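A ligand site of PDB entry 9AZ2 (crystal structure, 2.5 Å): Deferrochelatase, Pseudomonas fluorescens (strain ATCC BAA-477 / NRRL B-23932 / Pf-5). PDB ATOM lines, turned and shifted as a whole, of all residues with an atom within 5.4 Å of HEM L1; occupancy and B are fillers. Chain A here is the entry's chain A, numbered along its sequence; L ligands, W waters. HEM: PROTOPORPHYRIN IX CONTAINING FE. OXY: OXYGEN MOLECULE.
N of Phe 334 lies within hydrogen-bond range of O of Arg 239 (2.9 Å).
The backbone NH (N) of Ile 296 lies within hydrogen-bond range of the backbone carbonyl oxygen (O) of Ile 260, at 3.1 Å.
OD1 of Asn 195 lies within hydrogen-bond range of N of Leu 197 (2.9 Å).
O of Ile 241 sits at hydrogen-bond distance from N of Leu 332 (2.9 Å).
The backbone NH (N) of Arg 302 lies close to the side-chain amide oxygen (OD1) of Asn 300 (3.0 Å).
N of His 295 is in hydrogen-bond range of O of Ile 260, at 3.2 Å.
The side-chain amide oxygen of Asn 195 is in hydrogen-bond range of the backbone NH of Phe 199 (3.4 Å).
ND2 of Asn 205 sits at hydrogen-bond distance from O of Arg 313 (2.8 Å).
NE2 of His 295 binds FE of HEM L1.
The backbone NH (N) of Ser 203 lies within hydrogen-bond range of an oxygen (O1D) of HEM L1 (3.2 Å).
An oxygen (O2A) of HEM L1 is in salt-bridge range of the guanidinium group (NH2) of Arg 302, 2.7 Å away.
O2D of HEM L1 sits at hydrogen-bond distance from N of Ala 204 (2.9 Å).
O1D of HEM L1 lies within hydrogen-bond range of N of Gly 202 (2.7 Å).
An oxygen (O2) of OXY L2 is in hydrogen-bond range of the guanidinium group (NH1) of Arg 313.
An oxygen (O1D) of HEM L1 is in salt-bridge range of the guanidinium group (NH2) of Arg 313 (2.6 Å).
The side-chain amide nitrogen (ND2) of Asn 300 is in hydrogen-bond range of an oxygen (O1A) of HEM L1 (2.8 Å).
Water W2 lies within hydrogen-bond range of O2A of HEM L1, OH of Tyr 281, NE of Arg 302, O of Ile 296 and O of Asn 300.
Water W3 lies within hydrogen-bond range of NE of Arg 262 (2.9 Å) and O2A of HEM L1 (2.9 Å).
Water W1 lies within hydrogen-bond range of the guanidinium group of Arg 239 and the side-chain amide oxygen of Gln 349.
ND2 of Asn 195 touches CAC of HEM L1, at 3.2 Å.
Leu 197 touches HEM L1 (CD2 to CBC, 3.5 Å).
Phe 199 touches HEM L1.
Arg 200 touches HEM L1.
C of Asp 201 touches O1D of HEM L1 (3.8 Å).
CD1 of Ile 241 touches CBB of HEM L1, at 3.4 Å.
Asn 243 touches HEM L1.
CG2 of Ile 260 touches CMD of HEM L1, 3.6 Å away.
Arg 262 touches HEM L1.
Ile 296 touches HEM L1 (CG2 to CHA, 3.5 Å).
CB of Ala 299 touches C3A of HEM L1, at 3.5 Å.
Leu 332 touches HEM L1 (CD2 to C2C, 3.7 Å).
Phe 334 touches HEM L1 (CE1 to C3B, 3.4 Å).
CE1 of Phe 345 touches CAB of HEM L1 (3.8 Å).
Val 348 touches HEM L1.
Gln 349 touches HEM L1 (OE1 to CAB, 3.2 Å).
Leu 352 touches HEM L1 (CD1 to C2B, 3.6 Å).
Leu 361 touches HEM L1 (CD1 to CMC, 3.7 Å).
Hydrophobic or aromatic side chains that line HEM L1: Leu 197, Phe 199, Ala 204, Ile 241, Ile 260, His 295, Ile 296, Ala 299, Leu 332, Phe 334, Phe 345, Val 348, Leu 352 and Leu 361.
25 residues have an atom within 4 Å of HEM L1: Asn 195, Leu 197, Phe 199, Arg 200, Asp 201, Gly 202, Ser 203, Ala 204, Ile 241, Asn 243, Ile 260, Arg 262, His 295, Ile 296, Ala 299, Asn 300, Arg 302, Arg 313, Leu 332, Phe 334, Phe 345, Val 348, Gln 349, Leu 352 and Leu 361.
The nearest printed residue that does not touch HEM L1 is Ile 311 (4.2 Å).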
ATOM      1  N   ASN A 195     -16.797 -32.234  17.601  1.00  0.00           N
ATOM      2  CA  ASN A 195     -16.685 -31.018  18.400  1.00  0.00           C
ATOM      3  C   ASN A 195     -17.651 -31.069  19.577  1.00  0.00           C
ATOM      4  O   ASN A 195     -18.399 -32.035  19.765  1.00  0.00           O
ATOM      5  CB  ASN A 195     -16.903 -29.785  17.518  1.00  0.00           C
ATOM      6  CG  ASN A 195     -18.302 -29.710  16.914  1.00  0.00           C
ATOM      7  OD1 ASN A 195     -19.251 -30.336  17.398  1.00  0.00           O
ATOM      8  ND2 ASN A 195     -18.424 -28.936  15.847  1.00  0.00           N
ATOM      9  N   LEU A 197     -20.337 -29.707  19.981  1.00  0.00           N
ATOM     10  CA  LEU A 197     -21.727 -29.753  19.562  1.00  0.00           C
ATOM     11  C   LEU A 197     -22.168 -31.150  19.155  1.00  0.00           C
ATOM     12  O   LEU A 197     -23.325 -31.335  18.770  1.00  0.00           O
ATOM     13  CB  LEU A 197     -21.967 -28.774  18.401  1.00  0.00           C
ATOM     14  CG  LEU A 197     -22.738 -27.503  18.740  1.00  0.00           C
ATOM     15  CD1 LEU A 197     -22.166 -26.829  19.975  1.00  0.00           C
ATOM     16  CD2 LEU A 197     -22.758 -26.540  17.556  1.00  0.00           C
ATOM     17  N   PHE A 199     -21.101 -33.019  16.606  1.00  0.00           N
ATOM     18  CA  PHE A 199     -20.998 -33.315  15.186  1.00  0.00           C
ATOM     19  C   PHE A 199     -19.541 -33.529  14.784  1.00  0.00           C
ATOM     20  O   PHE A 199     -18.626 -32.930  15.354  1.00  0.00           O
ATOM     21  CB  PHE A 199     -21.605 -32.192  14.349  1.00  0.00           C
ATOM     22  CG  PHE A 199     -23.104 -32.153  14.367  1.00  0.00           C
ATOM     23  CD1 PHE A 199     -23.782 -31.659  15.466  1.00  0.00           C
ATOM     24  CD2 PHE A 199     -23.828 -32.620  13.284  1.00  0.00           C
ATOM     25  CE1 PHE A 199     -25.166 -31.624  15.478  1.00  0.00           C
ATOM     26  CE2 PHE A 199     -25.212 -32.585  13.296  1.00  0.00           C
ATOM     27  CZ  PHE A 199     -25.881 -32.087  14.394  1.00  0.00           C
ATOM     28  N   ARG A 200     -19.341 -34.390  13.786  1.00  0.00           N
ATOM     29  CA  ARG A 200     -18.018 -34.587  13.216  1.00  0.00           C
ATOM     30  C   ARG A 200     -17.546 -33.294  12.562  1.00  0.00           C
ATOM     31  O   ARG A 200     -18.286 -32.667  11.802  1.00  0.00           O
ATOM     32  CB  ARG A 200     -18.042 -35.723  12.197  1.00  0.00           C
ATOM     33  CG  ARG A 200     -18.518 -37.052  12.778  1.00  0.00           C
ATOM     34  CD  ARG A 200     -18.275 -38.209  11.815  1.00  0.00           C
ATOM     35  NE  ARG A 200     -19.155 -39.337  12.087  1.00  0.00           N
ATOM     36  CZ  ARG A 200     -19.060 -40.524  11.503  1.00  0.00           C
ATOM     37  NH1 ARG A 200     -18.132 -40.768  10.601  1.00  0.00           N
ATOM     38  NH2 ARG A 200     -19.918 -41.479  11.838  1.00  0.00           N
ATOM     39  N   ASP A 201     -16.315 -32.896  12.871  1.00  0.00           N
ATOM     40  CA  ASP A 201     -15.771 -31.611  12.459  1.00  0.00           C
ATOM     41  C   ASP A 201     -14.595 -31.843  11.513  1.00  0.00           C
ATOM     42  O   ASP A 201     -13.583 -32.435  11.916  1.00  0.00           O
ATOM     43  CB  ASP A 201     -15.340 -30.781  13.667  1.00  0.00           C
ATOM     44  CG  ASP A 201     -15.294 -29.306  13.377  1.00  0.00           C
ATOM     45  OD1 ASP A 201     -14.740 -28.924  12.321  1.00  0.00           O
ATOM     46  OD2 ASP A 201     -15.807 -28.523  14.202  1.00  0.00           O
ATOM     47  N   GLY A 202     -14.716 -31.359  10.287  1.00  0.00           N
ATOM     48  CA  GLY A 202     -13.665 -31.469   9.298  1.00  0.00           C
ATOM     49  C   GLY A 202     -13.902 -32.458   8.179  1.00  0.00           C
ATOM     50  O   GLY A 202     -12.965 -32.727   7.410  1.00  0.00           O
ATOM     51  N   SER A 203     -15.111 -33.003   8.060  1.00  0.00           N
ATOM     52  CA  SER A 203     -15.367 -34.035   7.049  1.00  0.00           C
ATOM     53  C   SER A 203     -15.094 -33.529   5.642  1.00  0.00           C
ATOM     54  O   SER A 203     -14.487 -34.229   4.827  1.00  0.00           O
ATOM     55  CB  SER A 203     -16.819 -34.529   7.163  1.00  0.00           C
ATOM     56  OG  SER A 203     -17.235 -34.570   8.512  1.00  0.00           O
ATOM     57  N   ALA A 204     -15.543 -32.312   5.327  1.00  0.00           N
ATOM     58  CA  ALA A 204     -15.409 -31.757   3.990  1.00  0.00           C
ATOM     59  C   ALA A 204     -14.087 -31.015   3.776  1.00  0.00           C
ATOM     60  O   ALA A 204     -13.973 -30.229   2.825  1.00  0.00           O
ATOM     61  CB  ALA A 204     -16.585 -30.817   3.694  1.00  0.00           C
ATOM     62  N   ASN A 205     -13.103 -31.249   4.636  1.00  0.00           N
ATOM     63  CA  ASN A 205     -11.785 -30.655   4.419  1.00  0.00           C
ATOM     64  C   ASN A 205     -11.193 -31.167   3.119  1.00  0.00           C
ATOM     65  O   ASN A 205     -11.398 -32.328   2.754  1.00  0.00           O
ATOM     66  CB  ASN A 205     -10.857 -30.987   5.586  1.00  0.00           C
ATOM     67  CG  ASN A 205     -10.688 -29.837   6.559  1.00  0.00           C
ATOM     68  OD1 ASN A 205     -10.927 -28.682   6.222  1.00  0.00           O
ATOM     69  ND2 ASN A 205     -10.271 -30.149   7.783  1.00  0.00           N
ATOM     70  N   ARG A 239     -10.225 -18.160  15.837  1.00  0.00           N
ATOM     71  CA  ARG A 239     -11.450 -17.620  16.416  1.00  0.00           C
ATOM     72  C   ARG A 239     -11.825 -18.466  17.628  1.00  0.00           C
ATOM     73  O   ARG A 239     -12.054 -19.673  17.487  1.00  0.00           O
ATOM     74  CB  ARG A 239     -12.591 -17.605  15.400  1.00  0.00           C
ATOM     75  CG  ARG A 239     -12.296 -16.843  14.121  1.00  0.00           C
ATOM     76  CD  ARG A 239     -12.774 -15.414  14.209  1.00  0.00           C
ATOM     77  NE  ARG A 239     -14.229 -15.325  14.072  1.00  0.00           N
ATOM     78  CZ  ARG A 239     -14.931 -14.210  14.254  1.00  0.00           C
ATOM     79  NH1 ARG A 239     -14.338 -13.066  14.582  1.00  0.00           N
ATOM     80  NH2 ARG A 239     -16.243 -14.248  14.111  1.00  0.00           N
ATOM     81  N   ILE A 241     -14.618 -19.385  19.655  1.00  0.00           N
ATOM     82  CA  ILE A 241     -16.065 -19.323  19.473  1.00  0.00           C
ATOM     83  C   ILE A 241     -16.731 -20.056  20.636  1.00  0.00           C
ATOM     84  O   ILE A 241     -16.523 -21.258  20.817  1.00  0.00           O
ATOM     85  CB  ILE A 241     -16.488 -19.943  18.127  1.00  0.00           C
ATOM     86  CG1 ILE A 241     -15.908 -19.124  16.982  1.00  0.00           C
ATOM     87  CG2 ILE A 241     -18.008 -20.004  18.027  1.00  0.00           C
ATOM     88  CD1 ILE A 241     -15.361 -19.962  15.877  1.00  0.00           C
ATOM     89  N   ASN A 243     -19.681 -21.848  22.727  1.00  0.00           N
ATOM     90  CA  ASN A 243     -20.827 -22.710  22.465  1.00  0.00           C
ATOM     91  C   ASN A 243     -21.792 -22.608  23.637  1.00  0.00           C
ATOM     92  O   ASN A 243     -21.397 -22.854  24.787  1.00  0.00           O
ATOM     93  CB  ASN A 243     -20.396 -24.166  22.254  1.00  0.00           C
ATOM     94  CG  ASN A 243     -19.866 -24.425  20.864  1.00  0.00           C
ATOM     95  OD1 ASN A 243     -20.026 -23.600  19.963  1.00  0.00           O
ATOM     96  ND2 ASN A 243     -19.227 -25.574  20.677  1.00  0.00           N
ATOM     97  N   ILE A 260     -26.948 -27.397  10.851  1.00  0.00           N
ATOM     98  CA  ILE A 260     -25.579 -27.671  10.413  1.00  0.00           C
ATOM     99  C   ILE A 260     -25.571 -28.142   8.963  1.00  0.00           C
ATOM    100  O   ILE A 260     -24.729 -27.723   8.168  1.00  0.00           O
ATOM    101  CB  ILE A 260     -24.918 -28.693  11.352  1.00  0.00           C
ATOM    102  CG1 ILE A 260     -24.714 -28.080  12.731  1.00  0.00           C
ATOM    103  CG2 ILE A 260     -23.611 -29.200  10.756  1.00  0.00           C
ATOM    104  CD1 ILE A 260     -23.603 -28.714  13.531  1.00  0.00           C
ATOM    105  N   ARG A 262     -25.888 -31.692   8.221  1.00  0.00           N
ATOM    106  CA  ARG A 262     -25.394 -33.051   8.171  1.00  0.00           C
ATOM    107  C   ARG A 262     -26.026 -33.861   9.296  1.00  0.00           C
ATOM    108  O   ARG A 262     -26.413 -33.310  10.334  1.00  0.00           O
ATOM    109  CB  ARG A 262     -23.865 -33.112   8.292  1.00  0.00           C
ATOM    110  CG  ARG A 262     -23.133 -32.568   7.078  1.00  0.00           C
ATOM    111  CD  ARG A 262     -21.717 -33.105   6.998  1.00  0.00           C
ATOM    112  NE  ARG A 262     -21.082 -32.808   5.724  1.00  0.00           N
ATOM    113  CZ  ARG A 262     -20.688 -33.725   4.855  1.00  0.00           C
ATOM    114  NH1 ARG A 262     -20.857 -35.015   5.091  1.00  0.00           N
ATOM    115  NH2 ARG A 262     -20.102 -33.336   3.725  1.00  0.00           N
ATOM    116  N   PRO A 279     -23.043 -33.170  -0.538  1.00  0.00           N
ATOM    117  CA  PRO A 279     -24.407 -32.982  -1.048  1.00  0.00           C
ATOM    118  C   PRO A 279     -24.417 -32.434  -2.463  1.00  0.00           C
ATOM    119  O   PRO A 279     -23.442 -31.860  -2.954  1.00  0.00           O
ATOM    120  CB  PRO A 279     -25.014 -31.991  -0.059  1.00  0.00           C
ATOM    121  CG  PRO A 279     -23.854 -31.254   0.511  1.00  0.00           C
ATOM    122  CD  PRO A 279     -22.705 -32.217   0.525  1.00  0.00           C
ATOM    123  N   TYR A 281     -26.198 -29.766  -4.381  1.00  0.00           N
ATOM    124  CA  TYR A 281     -27.024 -28.569  -4.229  1.00  0.00           C
ATOM    125  C   TYR A 281     -27.763 -28.217  -5.509  1.00  0.00           C
ATOM    126  O   TYR A 281     -28.846 -27.629  -5.448  1.00  0.00           O
ATOM    127  CB  TYR A 281     -26.160 -27.392  -3.776  1.00  0.00           C
ATOM    128  CG  TYR A 281     -25.609 -27.545  -2.384  1.00  0.00           C
ATOM    129  CD1 TYR A 281     -26.209 -28.382  -1.457  1.00  0.00           C
ATOM    130  CD2 TYR A 281     -24.481 -26.832  -1.980  1.00  0.00           C
ATOM    131  CE1 TYR A 281     -25.716 -28.517  -0.180  1.00  0.00           C
ATOM    132  CE2 TYR A 281     -23.964 -26.971  -0.704  1.00  0.00           C
ATOM    133  CZ  TYR A 281     -24.589 -27.809   0.196  1.00  0.00           C
ATOM    134  OH  TYR A 281     -24.085 -27.948   1.466  1.00  0.00           O
ATOM    135  N   HIS A 295     -25.218 -24.613   7.754  1.00  0.00           N
ATOM    136  CA  HIS A 295     -23.854 -24.165   7.983  1.00  0.00           C
ATOM    137  C   HIS A 295     -22.945 -24.553   6.819  1.00  0.00           C
ATOM    138  O   HIS A 295     -22.196 -23.725   6.288  1.00  0.00           O
ATOM    139  CB  HIS A 295     -23.321 -24.751   9.284  1.00  0.00           C
ATOM    140  CG  HIS A 295     -21.930 -24.328   9.624  1.00  0.00           C
ATOM    141  ND1 HIS A 295     -21.588 -23.021   9.879  1.00  0.00           N
ATOM    142  CD2 HIS A 295     -20.781 -25.043   9.732  1.00  0.00           C
ATOM    143  CE1 HIS A 295     -20.293 -22.944  10.132  1.00  0.00           C
ATOM    144  NE2 HIS A 295     -19.776 -24.159  10.048  1.00  0.00           N
ATOM    145  N   ILE A 296     -23.017 -25.817   6.377  1.00  0.00           N
ATOM    146  CA  ILE A 296     -22.139 -26.272   5.313  1.00  0.00           C
ATOM    147  C   ILE A 296     -22.572 -25.695   3.972  1.00  0.00           C
ATOM    148  O   ILE A 296     -21.723 -25.446   3.089  1.00  0.00           O
ATOM    149  CB  ILE A 296     -22.092 -27.818   5.273  1.00  0.00           C
ATOM    150  CG1 ILE A 296     -23.487 -28.394   5.003  1.00  0.00           C
ATOM    151  CG2 ILE A 296     -21.548 -28.358   6.574  1.00  0.00           C
ATOM    152  CD1 ILE A 296     -23.451 -29.722   4.280  1.00  0.00           C
ATOM    153  N   ALA A 299     -21.270 -22.118   4.085  1.00  0.00           N
ATOM    154  CA  ALA A 299     -19.817 -22.095   4.052  1.00  0.00           C
ATOM    155  C   ALA A 299     -19.245 -22.596   2.730  1.00  0.00           C
ATOM    156  O   ALA A 299     -18.080 -22.321   2.431  1.00  0.00           O
ATOM    157  CB  ALA A 299     -19.247 -22.925   5.207  1.00  0.00           C
ATOM    158  N   ASN A 300     -20.049 -23.313   1.945  1.00  0.00           N
ATOM    159  CA  ASN A 300     -19.573 -23.857   0.678  1.00  0.00           C
ATOM    160  C   ASN A 300     -20.747 -24.091  -0.265  1.00  0.00           C
ATOM    161  O   ASN A 300     -21.385 -25.156  -0.216  1.00  0.00           O
ATOM    162  CB  ASN A 300     -18.808 -25.162   0.906  1.00  0.00           C
ATOM    163  CG  ASN A 300     -18.133 -25.672  -0.354  1.00  0.00           C
ATOM    164  OD1 ASN A 300     -18.071 -24.979  -1.367  1.00  0.00           O
ATOM    165  ND2 ASN A 300     -17.628 -26.913  -0.297  1.00  0.00           N
ATOM    166  N   ARG A 302     -20.502 -24.866  -3.175  1.00  0.00           N
ATOM    167  CA  ARG A 302     -20.050 -25.926  -4.072  1.00  0.00           C
ATOM    168  C   ARG A 302     -20.310 -25.564  -5.529  1.00  0.00           C
ATOM    169  O   ARG A 302     -20.644 -26.417  -6.351  1.00  0.00           O
ATOM    170  CB  ARG A 302     -20.674 -27.269  -3.711  1.00  0.00           C
ATOM    171  CG  ARG A 302     -20.432 -27.666  -2.269  1.00  0.00           C
ATOM    172  CD  ARG A 302     -20.971 -29.051  -1.948  1.00  0.00           C
ATOM    173  NE  ARG A 302     -20.488 -29.521  -0.664  1.00  0.00           N
ATOM    174  CZ  ARG A 302     -19.317 -30.123  -0.468  1.00  0.00           C
ATOM    175  NH1 ARG A 302     -18.478 -30.332  -1.473  1.00  0.00           N
ATOM    176  NH2 ARG A 302     -18.976 -30.507   0.758  1.00  0.00           N
ATOM    177  N   ILE A 311     -11.080 -23.838   2.407  1.00  0.00           N
ATOM    178  CA  ILE A 311     -10.115 -23.647   3.482  1.00  0.00           C
ATOM    179  C   ILE A 311      -9.784 -24.995   4.099  1.00  0.00           C
ATOM    180  O   ILE A 311     -10.503 -25.981   3.930  1.00  0.00           O
ATOM    181  CB  ILE A 311     -10.633 -22.691   4.573  1.00  0.00           C
ATOM    182  CG1 ILE A 311     -11.902 -23.244   5.226  1.00  0.00           C
ATOM    183  CG2 ILE A 311     -10.878 -21.297   4.009  1.00  0.00           C
ATOM    184  CD1 ILE A 311     -12.370 -22.448   6.421  1.00  0.00           C
ATOM    185  N   ARG A 313      -9.511 -26.562   7.606  1.00  0.00           N
ATOM    186  CA  ARG A 313      -9.870 -26.349   9.003  1.00  0.00           C
ATOM    187  C   ARG A 313      -9.117 -27.321   9.893  1.00  0.00           C
ATOM    188  O   ARG A 313      -8.976 -28.504   9.571  1.00  0.00           O
ATOM    189  CB  ARG A 313     -11.380 -26.508   9.191  1.00  0.00           C
ATOM    190  CG  ARG A 313     -12.166 -25.272   8.789  1.00  0.00           C
ATOM    191  CD  ARG A 313     -13.653 -25.561   8.669  1.00  0.00           C
ATOM    192  NE  ARG A 313     -13.924 -26.653   7.741  1.00  0.00           N
ATOM    193  CZ  ARG A 313     -14.601 -27.748   8.055  1.00  0.00           C
ATOM    194  NH1 ARG A 313     -15.101 -27.927   9.267  1.00  0.00           N
ATOM    195  NH2 ARG A 313     -14.789 -28.691   7.134  1.00  0.00           N
ATOM    196  N   LEU A 332     -15.486 -23.996  20.515  1.00  0.00           N
ATOM    197  CA  LEU A 332     -14.582 -24.413  19.450  1.00  0.00           C
ATOM    198  C   LEU A 332     -13.403 -23.460  19.386  1.00  0.00           C
ATOM    199  O   LEU A 332     -13.582 -22.251  19.196  1.00  0.00           O
ATOM    200  CB  LEU A 332     -15.296 -24.461  18.108  1.00  0.00           C
ATOM    201  CG  LEU A 332     -14.523 -25.128  16.969  1.00  0.00           C
ATOM    202  CD1 LEU A 332     -14.430 -26.627  17.192  1.00  0.00           C
ATOM    203  CD2 LEU A 332     -15.158 -24.819  15.627  1.00  0.00           C
ATOM    204  N   PHE A 334     -11.329 -22.450  16.985  1.00  0.00           N
ATOM    205  CA  PHE A 334     -11.302 -22.517  15.530  1.00  0.00           C
ATOM    206  C   PHE A 334      -9.941 -22.090  15.008  1.00  0.00           C
ATOM    207  O   PHE A 334      -9.439 -21.010  15.337  1.00  0.00           O
ATOM    208  CB  PHE A 334     -12.399 -21.636  14.931  1.00  0.00           C
ATOM    209  CG  PHE A 334     -12.508 -21.731  13.444  1.00  0.00           C
ATOM    210  CD1 PHE A 334     -13.318 -22.696  12.859  1.00  0.00           C
ATOM    211  CD2 PHE A 334     -11.823 -20.859  12.615  1.00  0.00           C
ATOM    212  CE1 PHE A 334     -13.428 -22.785  11.479  1.00  0.00           C
ATOM    213  CE2 PHE A 334     -11.920 -20.948  11.241  1.00  0.00           C
ATOM    214  CZ  PHE A 334     -12.729 -21.911  10.670  1.00  0.00           C
ATOM    215  N   PHE A 345     -10.965 -17.489   4.835  1.00  0.00           N
ATOM    216  CA  PHE A 345     -11.828 -17.364   6.013  1.00  0.00           C
ATOM    217  C   PHE A 345     -12.727 -16.134   5.927  1.00  0.00           C
ATOM    218  O   PHE A 345     -13.911 -16.205   6.263  1.00  0.00           O
ATOM    219  CB  PHE A 345     -10.971 -17.307   7.282  1.00  0.00           C
ATOM    220  CG  PHE A 345     -11.731 -16.864   8.501  1.00  0.00           C
ATOM    221  CD1 PHE A 345     -12.510 -17.764   9.204  1.00  0.00           C
ATOM    222  CD2 PHE A 345     -11.673 -15.554   8.928  1.00  0.00           C
ATOM    223  CE1 PHE A 345     -13.217 -17.364  10.320  1.00  0.00           C
ATOM    224  CE2 PHE A 345     -12.374 -15.142  10.049  1.00  0.00           C
ATOM    225  CZ  PHE A 345     -13.151 -16.049  10.745  1.00  0.00           C
ATOM    226  N   VAL A 348     -15.628 -16.672   3.628  1.00  0.00           N
ATOM    227  CA  VAL A 348     -16.551 -17.702   4.122  1.00  0.00           C
ATOM    228  C   VAL A 348     -17.362 -17.172   5.293  1.00  0.00           C
ATOM    229  O   VAL A 348     -18.593 -17.317   5.336  1.00  0.00           O
ATOM    230  CB  VAL A 348     -15.780 -18.983   4.490  1.00  0.00           C
ATOM    231  CG1 VAL A 348     -16.702 -19.960   5.184  1.00  0.00           C
ATOM    232  CG2 VAL A 348     -15.169 -19.605   3.251  1.00  0.00           C
ATOM    233  N   GLN A 349     -16.688 -16.544   6.273  1.00  0.00           N
ATOM    234  CA  GLN A 349     -17.398 -15.996   7.421  1.00  0.00           C
ATOM    235  C   GLN A 349     -18.407 -14.929   7.002  1.00  0.00           C
ATOM    236  O   GLN A 349     -19.442 -14.760   7.664  1.00  0.00           O
ATOM    237  CB  GLN A 349     -16.393 -15.416   8.421  1.00  0.00           C
ATOM    238  CG  GLN A 349     -17.018 -14.907   9.708  1.00  0.00           C
ATOM    239  CD  GLN A 349     -17.875 -15.947  10.396  1.00  0.00           C
ATOM    240  OE1 GLN A 349     -17.408 -17.039  10.731  1.00  0.00           O
ATOM    241  NE2 GLN A 349     -19.144 -15.621  10.604  1.00  0.00           N
ATOM    242  N   LEU A 352     -21.440 -16.825   6.112  1.00  0.00           N
ATOM    243  CA  LEU A 352     -22.043 -17.407   7.305  1.00  0.00           C
ATOM    244  C   LEU A 352     -22.703 -16.361   8.200  1.00  0.00           C
ATOM    245  O   LEU A 352     -23.345 -16.745   9.181  1.00  0.00           O
ATOM    246  CB  LEU A 352     -20.999 -18.173   8.116  1.00  0.00           C
ATOM    247  CG  LEU A 352     -20.257 -19.311   7.405  1.00  0.00           C
ATOM    248  CD1 LEU A 352     -19.076 -19.781   8.252  1.00  0.00           C
ATOM    249  CD2 LEU A 352     -21.204 -20.460   7.110  1.00  0.00           C
ATOM    250  N   LEU A 357     -27.015 -20.987  12.919  1.00  0.00           N
ATOM    251  CA  LEU A 357     -26.073 -21.508  13.895  1.00  0.00           C
ATOM    252  C   LEU A 357     -25.605 -20.433  14.873  1.00  0.00           C
ATOM    253  O   LEU A 357     -25.145 -20.773  15.971  1.00  0.00           O
ATOM    254  CB  LEU A 357     -24.865 -22.118  13.177  1.00  0.00           C
ATOM    255  CG  LEU A 357     -23.855 -22.897  14.022  1.00  0.00           C
ATOM    256  CD1 LEU A 357     -24.527 -24.039  14.775  1.00  0.00           C
ATOM    257  CD2 LEU A 357     -22.710 -23.424  13.157  1.00  0.00           C
ATOM    258  N   LEU A 361     -23.652 -19.613  18.973  1.00  0.00           N
ATOM    259  CA  LEU A 361     -22.249 -19.256  18.821  1.00  0.00           C
ATOM    260  C   LEU A 361     -21.987 -17.854  19.351  1.00  0.00           C
ATOM    261  O   LEU A 361     -22.877 -16.996  19.342  1.00  0.00           O
ATOM    262  CB  LEU A 361     -21.803 -19.327  17.360  1.00  0.00           C
ATOM    263  CG  LEU A 361     -21.879 -20.692  16.678  1.00  0.00           C
ATOM    264  CD1 LEU A 361     -21.270 -20.619  15.285  1.00  0.00           C
ATOM    265  CD2 LEU A 361     -21.189 -21.754  17.515  1.00  0.00           C
HETATM  266  CHA HEM L   1     -18.357 -27.602   7.923  1.00  0.00           C
HETATM  267  CHB HEM L   1     -16.362 -23.173   7.763  1.00  0.00           C
HETATM  268  CHC HEM L   1     -17.417 -22.505  12.456  1.00  0.00           C
HETATM  269  CHD HEM L   1     -19.277 -26.986  12.661  1.00  0.00           C
HETATM  270  C1A HEM L   1     -17.704 -26.475   7.475  1.00  0.00           C
HETATM  271  C2A HEM L   1     -17.137 -26.277   6.156  1.00  0.00           C
HETATM  272  C3A HEM L   1     -16.585 -25.063   6.115  1.00  0.00           C
HETATM  273  C4A HEM L   1     -16.783 -24.440   7.405  1.00  0.00           C
HETATM  274  CMA HEM L   1     -15.877 -24.426   4.908  1.00  0.00           C
HETATM  275  CAA HEM L   1     -17.151 -27.277   4.978  1.00  0.00           C
HETATM  276  CBA HEM L   1     -18.504 -27.247   4.286  1.00  0.00           C
HETATM  277  CGA HEM L   1     -18.406 -27.950   2.965  1.00  0.00           C
HETATM  278  O1A HEM L   1     -17.313 -27.890   2.333  1.00  0.00           O
HETATM  279  O2A HEM L   1     -19.413 -28.556   2.522  1.00  0.00           O
HETATM  280  C1B HEM L   1     -16.466 -22.613   9.009  1.00  0.00           C
HETATM  281  C2B HEM L   1     -15.984 -21.302   9.393  1.00  0.00           C
HETATM  282  C3B HEM L   1     -16.273 -21.101  10.673  1.00  0.00           C
HETATM  283  C4B HEM L   1     -16.945 -22.286  11.182  1.00  0.00           C
HETATM  284  CMB HEM L   1     -15.269 -20.290   8.473  1.00  0.00           C
HETATM  285  CAB HEM L   1     -15.904 -19.803  11.431  1.00  0.00           C
HETATM  286  CBB HEM L   1     -16.299 -19.559  12.673  1.00  0.00           C
HETATM  287  C1C HEM L   1     -18.004 -23.667  12.928  1.00  0.00           C
HETATM  288  C2C HEM L   1     -18.443 -23.904  14.291  1.00  0.00           C
HETATM  289  C3C HEM L   1     -18.956 -25.144  14.349  1.00  0.00           C
HETATM  290  C4C HEM L   1     -18.865 -25.723  13.021  1.00  0.00           C
HETATM  291  CMC HEM L   1     -18.295 -22.848  15.417  1.00  0.00           C
HETATM  292  CAC HEM L   1     -19.564 -25.913  15.552  1.00  0.00           C
HETATM  293  CBC HEM L   1     -19.560 -25.471  16.812  1.00  0.00           C
HETATM  294  C1D HEM L   1     -19.190 -27.541  11.401  1.00  0.00           C
HETATM  295  C2D HEM L   1     -19.621 -28.880  11.027  1.00  0.00           C
HETATM  296  C3D HEM L   1     -19.370 -29.055   9.730  1.00  0.00           C
HETATM  297  C4D HEM L   1     -18.769 -27.843   9.220  1.00  0.00           C
HETATM  298  CMD HEM L   1     -20.249 -29.922  11.976  1.00  0.00           C
HETATM  299  CAD HEM L   1     -19.678 -30.350   8.933  1.00  0.00           C
HETATM  300  CBD HEM L   1     -18.469 -31.284   8.924  1.00  0.00           C
HETATM  301  CGD HEM L   1     -17.392 -30.704   8.046  1.00  0.00           C
HETATM  302  O1D HEM L   1     -16.410 -30.151   8.607  1.00  0.00           O
HETATM  303  O2D HEM L   1     -17.522 -30.784   6.795  1.00  0.00           O
HETATM  304  NA  HEM L   1     -17.463 -25.330   8.208  1.00  0.00           N
HETATM  305  NB  HEM L   1     -17.048 -23.186  10.134  1.00  0.00           N
HETATM  306  NC  HEM L   1     -18.276 -24.799  12.180  1.00  0.00           N
HETATM  307  ND  HEM L   1     -18.677 -26.940  10.275  1.00  0.00           N
HETATM  308 FE   HEM L   1     -17.848 -25.060  10.200  1.00  0.00          FE
HETATM  309  O1  OXY L   2     -14.559 -26.057  12.181  1.00  0.00           O
HETATM  310  O2  OXY L   2     -15.483 -25.864  11.433  1.00  0.00           O
HETATM  311  O   HOH W   1     -16.473 -16.650  13.398  1.00  0.00           O
HETATM  312  O   HOH W   2     -21.361 -27.776   1.272  1.00  0.00           O
HETATM  313  O   HOH W   3     -19.835 -30.537   4.534  1.00  0.00           O
